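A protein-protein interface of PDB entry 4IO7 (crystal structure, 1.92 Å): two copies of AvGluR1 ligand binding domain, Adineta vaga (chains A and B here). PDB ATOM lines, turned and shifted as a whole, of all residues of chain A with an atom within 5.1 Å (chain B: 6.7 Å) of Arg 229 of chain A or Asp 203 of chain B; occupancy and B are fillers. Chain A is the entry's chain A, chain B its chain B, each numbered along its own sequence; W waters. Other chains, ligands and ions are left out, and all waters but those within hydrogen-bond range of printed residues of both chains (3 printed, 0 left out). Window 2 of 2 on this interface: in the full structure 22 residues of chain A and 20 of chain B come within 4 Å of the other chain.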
ATOM      1  N   ILE A 225     -11.788 -28.022 -27.308  1.00  0.00           N
ATOM      2  CA  ILE A 225     -11.547 -26.584 -27.282  1.00  0.00           C
ATOM      3  C   ILE A 225     -12.822 -25.772 -27.330  1.00  0.00           C
ATOM      4  O   ILE A 225     -12.980 -24.816 -26.579  1.00  0.00           O
ATOM      5  CB  ILE A 225     -10.662 -26.144 -28.467  1.00  0.00           C
ATOM      6  CG1 ILE A 225      -9.260 -26.719 -28.275  1.00  0.00           C
ATOM      7  CG2 ILE A 225     -10.593 -24.648 -28.569  1.00  0.00           C
ATOM      8  CD1 ILE A 225      -8.453 -26.601 -29.516  1.00  0.00           C
ATOM      9  N   LEU A 226     -13.732 -26.133 -28.230  1.00  0.00           N
ATOM     10  CA  LEU A 226     -14.991 -25.393 -28.344  1.00  0.00           C
ATOM     11  C   LEU A 226     -15.798 -25.550 -27.051  1.00  0.00           C
ATOM     12  O   LEU A 226     -16.426 -24.612 -26.593  1.00  0.00           O
ATOM     13  CB  LEU A 226     -15.791 -25.859 -29.587  1.00  0.00           C
ATOM     14  CG  LEU A 226     -15.095 -25.461 -30.885  1.00  0.00           C
ATOM     15  CD1 LEU A 226     -15.590 -26.282 -32.079  1.00  0.00           C
ATOM     16  CD2 LEU A 226     -15.321 -23.943 -31.109  1.00  0.00           C
ATOM     17  N   SER A 227     -15.754 -26.719 -26.437  1.00  0.00           N
ATOM     18  CA  SER A 227     -16.448 -26.916 -25.181  1.00  0.00           C
ATOM     19  C   SER A 227     -15.894 -25.982 -24.056  1.00  0.00           C
ATOM     20  O   SER A 227     -16.677 -25.354 -23.317  1.00  0.00           O
ATOM     21  CB  SER A 227     -16.416 -28.393 -24.776  1.00  0.00           C
ATOM     22  OG  SER A 227     -17.006 -28.580 -23.502  1.00  0.00           O
ATOM     23  N   LEU A 228     -14.579 -25.896 -23.946  1.00  0.00           N
ATOM     24  CA  LEU A 228     -13.927 -24.947 -23.015  1.00  0.00           C
ATOM     25  C   LEU A 228     -14.346 -23.492 -23.292  1.00  0.00           C
ATOM     26  O   LEU A 228     -14.511 -22.692 -22.362  1.00  0.00           O
ATOM     27  CB  LEU A 228     -12.422 -25.095 -23.090  1.00  0.00           C
ATOM     28  CG  LEU A 228     -11.805 -26.400 -22.556  1.00  0.00           C
ATOM     29  CD1 LEU A 228     -10.291 -26.368 -22.616  1.00  0.00           C
ATOM     30  CD2 LEU A 228     -12.298 -26.723 -21.122  1.00  0.00           C
ATOM     31  N   ARG A 229     -14.514 -23.122 -24.546  1.00  0.00           N
ATOM     32  CA  ARG A 229     -15.005 -21.780 -24.810  1.00  0.00           C
ATOM     33  C   ARG A 229     -16.401 -21.676 -24.251  1.00  0.00           C
ATOM     34  O   ARG A 229     -16.708 -20.833 -23.395  1.00  0.00           O
ATOM     35  CB  ARG A 229     -15.032 -21.453 -26.303  1.00  0.00           C
ATOM     36  CG  ARG A 229     -15.755 -20.119 -26.572  1.00  0.00           C
ATOM     37  CD  ARG A 229     -15.997 -19.836 -28.036  1.00  0.00           C
ATOM     38  NE  ARG A 229     -17.123 -20.565 -28.636  1.00  0.00           N
ATOM     39  CZ  ARG A 229     -18.407 -20.448 -28.294  1.00  0.00           C
ATOM     40  NH1 ARG A 229     -18.790 -19.647 -27.301  1.00  0.00           N
ATOM     41  NH2 ARG A 229     -19.321 -21.166 -28.955  1.00  0.00           N
ATOM     42  N   GLU A 230     -17.264 -22.558 -24.739  1.00  0.00           N
ATOM     43  CA  GLU A 230     -18.669 -22.454 -24.433  1.00  0.00           C
ATOM     44  C   GLU A 230     -18.982 -22.395 -22.954  1.00  0.00           C
ATOM     45  O   GLU A 230     -19.878 -21.678 -22.520  1.00  0.00           O
ATOM     46  CB  GLU A 230     -19.405 -23.637 -25.085  1.00  0.00           C
ATOM     47  CG  GLU A 230     -19.462 -23.445 -26.611  1.00  0.00           C
ATOM     48  CD  GLU A 230     -19.764 -24.725 -27.379  1.00  0.00           C
ATOM     49  OE1 GLU A 230     -20.039 -25.766 -26.736  1.00  0.00           O
ATOM     50  OE2 GLU A 230     -19.618 -24.697 -28.628  1.00  0.00           O
ATOM     51  N   THR A 231     -18.263 -23.167 -22.171  1.00  0.00           N
ATOM     52  CA  THR A 231     -18.518 -23.194 -20.750  1.00  0.00           C
ATOM     53  C   THR A 231     -17.764 -22.097 -19.976  1.00  0.00           C
ATOM     54  O   THR A 231     -17.839 -22.061 -18.760  1.00  0.00           O
ATOM     55  CB  THR A 231     -18.190 -24.581 -20.175  1.00  0.00           C
ATOM     56  OG1 THR A 231     -16.801 -24.869 -20.355  1.00  0.00           O
ATOM     57  CG2 THR A 231     -19.019 -25.650 -20.880  1.00  0.00           C
ATOM     58  N   GLY A 232     -17.044 -21.230 -20.672  1.00  0.00           N
ATOM     59  CA  GLY A 232     -16.393 -20.078 -20.046  1.00  0.00           C
ATOM     60  C   GLY A 232     -14.982 -20.293 -19.500  1.00  0.00           C
ATOM     61  O   GLY A 232     -14.409 -19.398 -18.858  1.00  0.00           O
ATOM     62  N   ILE A 233     -14.408 -21.464 -19.740  1.00  0.00           N
ATOM     63  CA  ILE A 233     -13.101 -21.791 -19.172  1.00  0.00           C
ATOM     64  C   ILE A 233     -12.009 -20.943 -19.822  1.00  0.00           C
ATOM     65  O   ILE A 233     -11.092 -20.457 -19.145  1.00  0.00           O
ATOM     66  CB  ILE A 233     -12.748 -23.303 -19.280  1.00  0.00           C
ATOM     67  CG1 ILE A 233     -13.725 -24.206 -18.469  1.00  0.00           C
ATOM     68  CG2 ILE A 233     -11.307 -23.556 -18.865  1.00  0.00           C
ATOM     69  CD1 ILE A 233     -13.985 -23.820 -17.041  1.00  0.00           C
ATOM     70  N   LEU A 234     -12.066 -20.754 -21.137  1.00  0.00           N
ATOM     71  CA  LEU A 234     -11.045 -19.930 -21.770  1.00  0.00           C
ATOM     72  C   LEU A 234     -11.100 -18.484 -21.235  1.00  0.00           C
ATOM     73  O   LEU A 234     -10.053 -17.872 -20.999  1.00  0.00           O
ATOM     74  CB  LEU A 234     -11.129 -19.993 -23.309  1.00  0.00           C
ATOM     75  CG  LEU A 234     -11.000 -21.405 -23.913  1.00  0.00           C
ATOM     76  CD1 LEU A 234     -11.092 -21.390 -25.482  1.00  0.00           C
ATOM     77  CD2 LEU A 234      -9.715 -22.079 -23.451  1.00  0.00           C
ATOM     78  N   THR B  87     -22.135 -20.116 -36.802  1.00  0.00           N
ATOM     79  CA  THR B  87     -21.313 -20.131 -35.631  1.00  0.00           C
ATOM     80  C   THR B  87     -20.671 -21.494 -35.469  1.00  0.00           C
ATOM     81  O   THR B  87     -21.301 -22.534 -35.631  1.00  0.00           O
ATOM     82  CB  THR B  87     -22.151 -19.782 -34.405  1.00  0.00           C
ATOM     83  OG1 THR B  87     -22.753 -18.504 -34.623  1.00  0.00           O
ATOM     84  CG2 THR B  87     -21.328 -19.746 -33.109  1.00  0.00           C
ATOM     85  N   VAL B  88     -19.396 -21.465 -35.121  1.00  0.00           N
ATOM     86  CA  VAL B  88     -18.697 -22.707 -34.856  1.00  0.00           C
ATOM     87  C   VAL B  88     -19.041 -23.165 -33.434  1.00  0.00           C
ATOM     88  O   VAL B  88     -18.791 -22.425 -32.469  1.00  0.00           O
ATOM     89  CB  VAL B  88     -17.168 -22.496 -34.996  1.00  0.00           C
ATOM     90  CG1 VAL B  88     -16.440 -23.823 -34.764  1.00  0.00           C
ATOM     91  CG2 VAL B  88     -16.839 -21.918 -36.394  1.00  0.00           C
ATOM     92  N   THR B  89     -19.633 -24.361 -33.287  1.00  0.00           N
ATOM     93  CA  THR B  89     -19.994 -24.864 -31.956  1.00  0.00           C
ATOM     94  C   THR B  89     -19.458 -26.274 -31.777  1.00  0.00           C
ATOM     95  O   THR B  89     -19.209 -26.990 -32.769  1.00  0.00           O
ATOM     96  CB  THR B  89     -21.543 -24.907 -31.699  1.00  0.00           C
ATOM     97  OG1 THR B  89     -22.095 -25.973 -32.472  1.00  0.00           O
ATOM     98  CG2 THR B  89     -22.204 -23.573 -32.052  1.00  0.00           C
ATOM     99  N   SER B  90     -19.323 -26.689 -30.531  1.00  0.00           N
ATOM    100  CA  SER B  90     -18.810 -28.034 -30.226  1.00  0.00           C
ATOM    101  C   SER B  90     -19.723 -29.140 -30.779  1.00  0.00           C
ATOM    102  O   SER B  90     -19.247 -30.122 -31.353  1.00  0.00           O
ATOM    103  CB  SER B  90     -18.586 -28.232 -28.734  1.00  0.00           C
ATOM    104  OG  SER B  90     -19.757 -28.111 -27.961  1.00  0.00           O
ATOM    105  N   ASN B 105     -17.299 -13.135 -33.466  1.00  0.00           N
ATOM    106  CA  ASN B 105     -18.730 -13.008 -33.261  1.00  0.00           C
ATOM    107  C   ASN B 105     -19.047 -12.950 -31.776  1.00  0.00           C
ATOM    108  O   ASN B 105     -18.251 -13.380 -30.940  1.00  0.00           O
ATOM    109  CB  ASN B 105     -19.486 -14.188 -33.896  1.00  0.00           C
ATOM    110  CG  ASN B 105     -20.997 -14.007 -33.849  1.00  0.00           C
ATOM    111  OD1 ASN B 105     -21.511 -12.950 -34.192  1.00  0.00           O
ATOM    112  ND2 ASN B 105     -21.708 -15.023 -33.385  1.00  0.00           N
ATOM    113  N   SER B 106     -20.216 -12.415 -31.470  1.00  0.00           N
ATOM    114  CA  SER B 106     -20.785 -12.457 -30.121  1.00  0.00           C
ATOM    115  C   SER B 106     -22.255 -12.171 -30.329  1.00  0.00           C
ATOM    116  O   SER B 106     -22.657 -11.894 -31.459  1.00  0.00           O
ATOM    117  CB  SER B 106     -20.142 -11.386 -29.226  1.00  0.00           C
ATOM    118  OG  SER B 106     -20.366 -10.072 -29.736  1.00  0.00           O
ATOM    119  N   MET B 107     -23.052 -12.248 -29.261  1.00  0.00           N
ATOM    120  CA  MET B 107     -24.467 -11.954 -29.352  1.00  0.00           C
ATOM    121  C   MET B 107     -24.810 -10.747 -28.520  1.00  0.00           C
ATOM    122  O   MET B 107     -24.090 -10.412 -27.571  1.00  0.00           O
ATOM    123  CB  MET B 107     -25.296 -13.163 -28.923  1.00  0.00           C
ATOM    124  CG  MET B 107     -25.263 -14.289 -29.948  1.00  0.00           C
ATOM    125  SD  MET B 107     -26.433 -15.589 -29.534  1.00  0.00           S
ATOM    126  CE  MET B 107     -25.473 -16.422 -28.269  1.00  0.00           C
ATOM    127  N   ALA B 140     -27.244 -21.093 -32.451  1.00  0.00           N
ATOM    128  CA  ALA B 140     -26.343 -20.939 -31.323  1.00  0.00           C
ATOM    129  C   ALA B 140     -26.982 -20.155 -30.194  1.00  0.00           C
ATOM    130  O   ALA B 140     -26.661 -20.331 -29.028  1.00  0.00           O
ATOM    131  CB  ALA B 140     -25.076 -20.232 -31.783  1.00  0.00           C
ATOM    132  N   GLY B 141     -27.884 -19.261 -30.530  1.00  0.00           N
ATOM    133  CA  GLY B 141     -28.602 -18.544 -29.496  1.00  0.00           C
ATOM    134  C   GLY B 141     -29.512 -19.449 -28.683  1.00  0.00           C
ATOM    135  O   GLY B 141     -29.653 -19.277 -27.463  1.00  0.00           O
ATOM    136  N   ASP B 143     -28.814 -22.609 -28.169  1.00  0.00           N
ATOM    137  CA  ASP B 143     -27.855 -23.397 -27.353  1.00  0.00           C
ATOM    138  C   ASP B 143     -27.490 -22.634 -26.094  1.00  0.00           C
ATOM    139  O   ASP B 143     -27.510 -23.183 -24.989  1.00  0.00           O
ATOM    140  CB  ASP B 143     -26.547 -23.687 -28.094  1.00  0.00           C
ATOM    141  CG  ASP B 143     -26.742 -24.423 -29.402  1.00  0.00           C
ATOM    142  OD1 ASP B 143     -27.736 -25.156 -29.547  1.00  0.00           O
ATOM    143  OD2 ASP B 143     -25.854 -24.296 -30.282  1.00  0.00           O
ATOM    144  N   TYR B 144     -27.153 -21.360 -26.270  1.00  0.00           N
ATOM    145  CA  TYR B 144     -26.768 -20.502 -25.159  1.00  0.00           C
ATOM    146  C   TYR B 144     -27.909 -20.402 -24.133  1.00  0.00           C
ATOM    147  O   TYR B 144     -27.710 -20.601 -22.927  1.00  0.00           O
ATOM    148  CB  TYR B 144     -26.368 -19.111 -25.661  1.00  0.00           C
ATOM    149  CG  TYR B 144     -26.044 -18.156 -24.529  1.00  0.00           C
ATOM    150  CD1 TYR B 144     -27.031 -17.398 -23.938  1.00  0.00           C
ATOM    151  CD2 TYR B 144     -24.748 -18.035 -24.048  1.00  0.00           C
ATOM    152  CE1 TYR B 144     -26.751 -16.544 -22.895  1.00  0.00           C
ATOM    153  CE2 TYR B 144     -24.457 -17.187 -22.997  1.00  0.00           C
ATOM    154  CZ  TYR B 144     -25.469 -16.453 -22.423  1.00  0.00           C
ATOM    155  OH  TYR B 144     -25.189 -15.589 -21.392  1.00  0.00           O
ATOM    156  N   ARG B 147     -28.323 -23.612 -22.181  1.00  0.00           N
ATOM    157  CA  ARG B 147     -27.195 -23.857 -21.282  1.00  0.00           C
ATOM    158  C   ARG B 147     -27.133 -22.879 -20.104  1.00  0.00           C
ATOM    159  O   ARG B 147     -26.896 -23.294 -18.968  1.00  0.00           O
ATOM    160  CB  ARG B 147     -25.867 -23.813 -22.067  1.00  0.00           C
ATOM    161  CG  ARG B 147     -24.625 -24.004 -21.202  1.00  0.00           C
ATOM    162  CD  ARG B 147     -23.327 -24.060 -22.035  1.00  0.00           C
ATOM    163  NE  ARG B 147     -23.038 -22.790 -22.693  1.00  0.00           N
ATOM    164  CZ  ARG B 147     -23.128 -22.568 -23.998  1.00  0.00           C
ATOM    165  NH1 ARG B 147     -23.495 -23.530 -24.849  1.00  0.00           N
ATOM    166  NH2 ARG B 147     -22.854 -21.366 -24.458  1.00  0.00           N
ATOM    167  N   ASP B 201     -22.304  -7.702 -24.650  1.00  0.00           N
ATOM    168  CA  ASP B 201     -22.395  -8.823 -25.578  1.00  0.00           C
ATOM    169  C   ASP B 201     -21.962 -10.088 -24.854  1.00  0.00           C
ATOM    170  O   ASP B 201     -21.421 -10.017 -23.754  1.00  0.00           O
ATOM    171  CB  ASP B 201     -21.622  -8.576 -26.876  1.00  0.00           C
ATOM    172  CG  ASP B 201     -20.135  -8.466 -26.673  1.00  0.00           C
ATOM    173  OD1 ASP B 201     -19.658  -8.634 -25.534  1.00  0.00           O
ATOM    174  OD2 ASP B 201     -19.444  -8.218 -27.682  1.00  0.00           O
ATOM    175  N   PHE B 202     -22.297 -11.239 -25.421  1.00  0.00           N
ATOM    176  CA  PHE B 202     -22.079 -12.513 -24.751  1.00  0.00           C
ATOM    177  C   PHE B 202     -21.848 -13.582 -25.779  1.00  0.00           C
ATOM    178  O   PHE B 202     -22.105 -13.367 -26.939  1.00  0.00           O
ATOM    179  CB  PHE B 202     -23.278 -12.892 -23.854  1.00  0.00           C
ATOM    180  CG  PHE B 202     -24.616 -12.870 -24.559  1.00  0.00           C
ATOM    181  CD1 PHE B 202     -25.234 -11.665 -24.844  1.00  0.00           C
ATOM    182  CD2 PHE B 202     -25.274 -14.073 -24.903  1.00  0.00           C
ATOM    183  CE1 PHE B 202     -26.492 -11.636 -25.476  1.00  0.00           C
ATOM    184  CE2 PHE B 202     -26.515 -14.059 -25.533  1.00  0.00           C
ATOM    185  CZ  PHE B 202     -27.127 -12.837 -25.828  1.00  0.00           C
ATOM    186  N   ASP B 203     -21.374 -14.732 -25.326  1.00  0.00           N
ATOM    187  CA  ASP B 203     -21.124 -15.882 -26.157  1.00  0.00           C
ATOM    188  C   ASP B 203     -20.110 -15.572 -27.259  1.00  0.00           C
ATOM    189  O   ASP B 203     -20.385 -15.785 -28.440  1.00  0.00           O
ATOM    190  CB  ASP B 203     -22.424 -16.421 -26.760  1.00  0.00           C
ATOM    191  CG  ASP B 203     -22.319 -17.896 -27.140  1.00  0.00           C
ATOM    192  OD1 ASP B 203     -21.629 -18.636 -26.421  1.00  0.00           O
ATOM    193  OD2 ASP B 203     -22.906 -18.332 -28.143  1.00  0.00           O
ATOM    194  N   LYS B 204     -18.936 -15.076 -26.872  1.00  0.00           N
ATOM    195  CA  LYS B 204     -17.900 -14.787 -27.859  1.00  0.00           C
ATOM    196  C   LYS B 204     -17.590 -16.057 -28.610  1.00  0.00           C
ATOM    197  O   LYS B 204     -17.449 -17.123 -28.011  1.00  0.00           O
ATOM    198  CB  LYS B 204     -16.647 -14.229 -27.195  1.00  0.00           C
ATOM    199  CG  LYS B 204     -16.864 -12.872 -26.571  1.00  0.00           C
ATOM    200  CD  LYS B 204     -15.975 -12.653 -25.361  1.00  0.00           C
ATOM    201  CE  LYS B 204     -16.467 -11.469 -24.529  1.00  0.00           C
ATOM    202  NZ  LYS B 204     -16.307 -10.167 -25.237  1.00  0.00           N
ATOM    203  N   SER B 205     -17.501 -15.949 -29.929  1.00  0.00           N
ATOM    204  CA  SER B 205     -17.462 -17.128 -30.784  1.00  0.00           C
ATOM    205  C   SER B 205     -16.894 -16.729 -32.147  1.00  0.00           C
ATOM    206  O   SER B 205     -16.316 -15.643 -32.285  1.00  0.00           O
ATOM    207  CB  SER B 205     -18.879 -17.691 -30.906  1.00  0.00           C
ATOM    208  OG  SER B 205     -19.796 -16.653 -31.255  1.00  0.00           O
ATOM    209  N   THR B 206     -17.036 -17.582 -33.152  1.00  0.00           N
ATOM    210  CA  THR B 206     -16.491 -17.281 -34.485  1.00  0.00           C
ATOM    211  C   THR B 206     -17.449 -17.860 -35.508  1.00  0.00           C
ATOM    212  O   THR B 206     -18.237 -18.745 -35.186  1.00  0.00           O
ATOM    213  CB  THR B 206     -15.108 -17.970 -34.743  1.00  0.00           C
ATOM    214  OG1 THR B 206     -15.231 -19.374 -34.462  1.00  0.00           O
ATOM    215  CG2 THR B 206     -14.019 -17.381 -33.873  1.00  0.00           C
HETATM  216  O   HOH W   1     -17.512 -20.126 -31.608  1.00  0.00           O
HETATM  217  O   HOH W   2     -22.354 -26.947 -28.748  1.00  0.00           O
HETATM  218  O   HOH W   3     -22.119 -20.758 -29.576  1.00  0.00           O
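The backbone carbonyl oxygen (O) of Ser 227 of chain A sits at hydrogen-bond distance from the side-chain hydroxyl (OG1) of Thr 231 of chain A (3.0 Å).
The backbone NH (N) of Val 88 of chain B sits at hydrogen-bond distance from the backbone carbonyl oxygen (O) of Thr 206 of chain B, at 3.0 Å.
O of Asn 105 of chain B lies within hydrogen-bond range of N of Ser 205 of chain B, at 2.9 Å.
The guanidinium group (NH2) of Arg 147 of chain B lies within salt-bridge range of the side-chain carboxylate (OD1) of Asp 203 of chain B, at 3.6 Å.
OD1 of Asp 201 of chain B is in salt-bridge range of NZ of Lys 204 of chain B.
O of Asp 203 of chain B sits at hydrogen-bond distance from OG of Ser 205 of chain B (3.0 Å).
Water W1 lies within hydrogen-bond range of the backbone carbonyl oxygen (O) of Val 88 of chain B (2.8 Å), the backbone NH (N) of Thr 206 of chain B (3.0 Å) and the guanidinium group (NE) of Arg 229 of chain A (3.0 Å).
Water W3 bridges NH2 of Arg 229 of chain A (2.9 Å) and OD2 of Asp 203 of chain B (2.9 Å).
Water W2 lies within hydrogen-bond range of the side-chain hydroxyl of Ser 90 of chain B and the side-chain carboxylate of Glu 230 of chain A.
Of the printed residues of chain B, Arg 229 of chain A touches Val 88, Asp 203, Lys 204 and Ser 205.
Printed residues of chain A within 4 Å of Asp 203 of chain B: Arg 229.
Of the printed residues of chain A, Ser 90 of chain B touches Leu 226, Ser 227 and Glu 230.
Printed residues of chain B within 4 Å of Glu 230 of chain A: Thr 89, Ser 90 and Arg 147.
Of the printed residues of chain B, Leu 226 of chain A touches Val 88, Thr 89 and Ser 90.
Of the printed residues of chain A, Ser 205 of chain B touches Arg 229.
Thr 206 of chain B touches none of the printed residues of chain A.
Thr 231 of chain A touches none of the printed residues of chain B.
The nearest printed residue of chain A that does not touch Asp 203 of chain B is Glu 230 of chain A (5.2 Å).
The nearest printed residue of chain B that does not touch Glu 230 of chain A is Val 88 of chain B (4.5 Å).
No position is printed for both chains.
Of the 11 pairs that touch across the chains among the printed residues, none has its exchanged pair printed and touching as well.
Hydrophobic or aromatic side chains of chain B within 4 Å of the printed part of chain A: Val 88.
Printed residues of chain A that touch a printed residue of chain B: Leu 226, Ser 227, Arg 229 and Glu 230.
Hydrophobic or aromatic side chains of chain A within 4 Å of the printed part of chain B: Leu 226.
Along chain A the printed residues that touch a printed residue of chain B span positions 226 to 230.
Among the printed residues, 11 pairs touch across the chains.
Among the printed residues, pairs that only touch across the chains: Glu 230 of chain A with Thr 89 of chain B (3.4 Å), Leu 226 of chain A with Val 88 of chain B (3.7 Å), Leu 226 of chain A with Ser 90 of chain B (3.7 Å), Leu 226 of chain A with Thr 89 of chain B (3.8 Å), Arg 229 of chain A with Val 88 of chain B (3.8 Å), Arg 229 of chain A with Ser 205 of chain B (3.8 Å) and Ser 227 of chain A with Ser 90 of chain B (3.9 Å).
The side-chain carboxylate (OD1) of Asp 203 of chain B lies within salt-bridge range of the guanidinium group (NH1) of Arg 229 of chain A, at 3.1 Å.
The backbone carbonyl oxygen (O) of Lys 204 of chain B lies within hydrogen-bond range of the guanidinium group (NH1) of Arg 229 of chain A.
The side-chain hydroxyl (OG) of Ser 90 of chain B sits at hydrogen-bond distance from the side-chain carboxylate (OE1) of Glu 230 of chain A, at 2.7 Å.
O of Glu 230 of chain A is in hydrogen-bond range of NE of Arg 147 of chain B.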
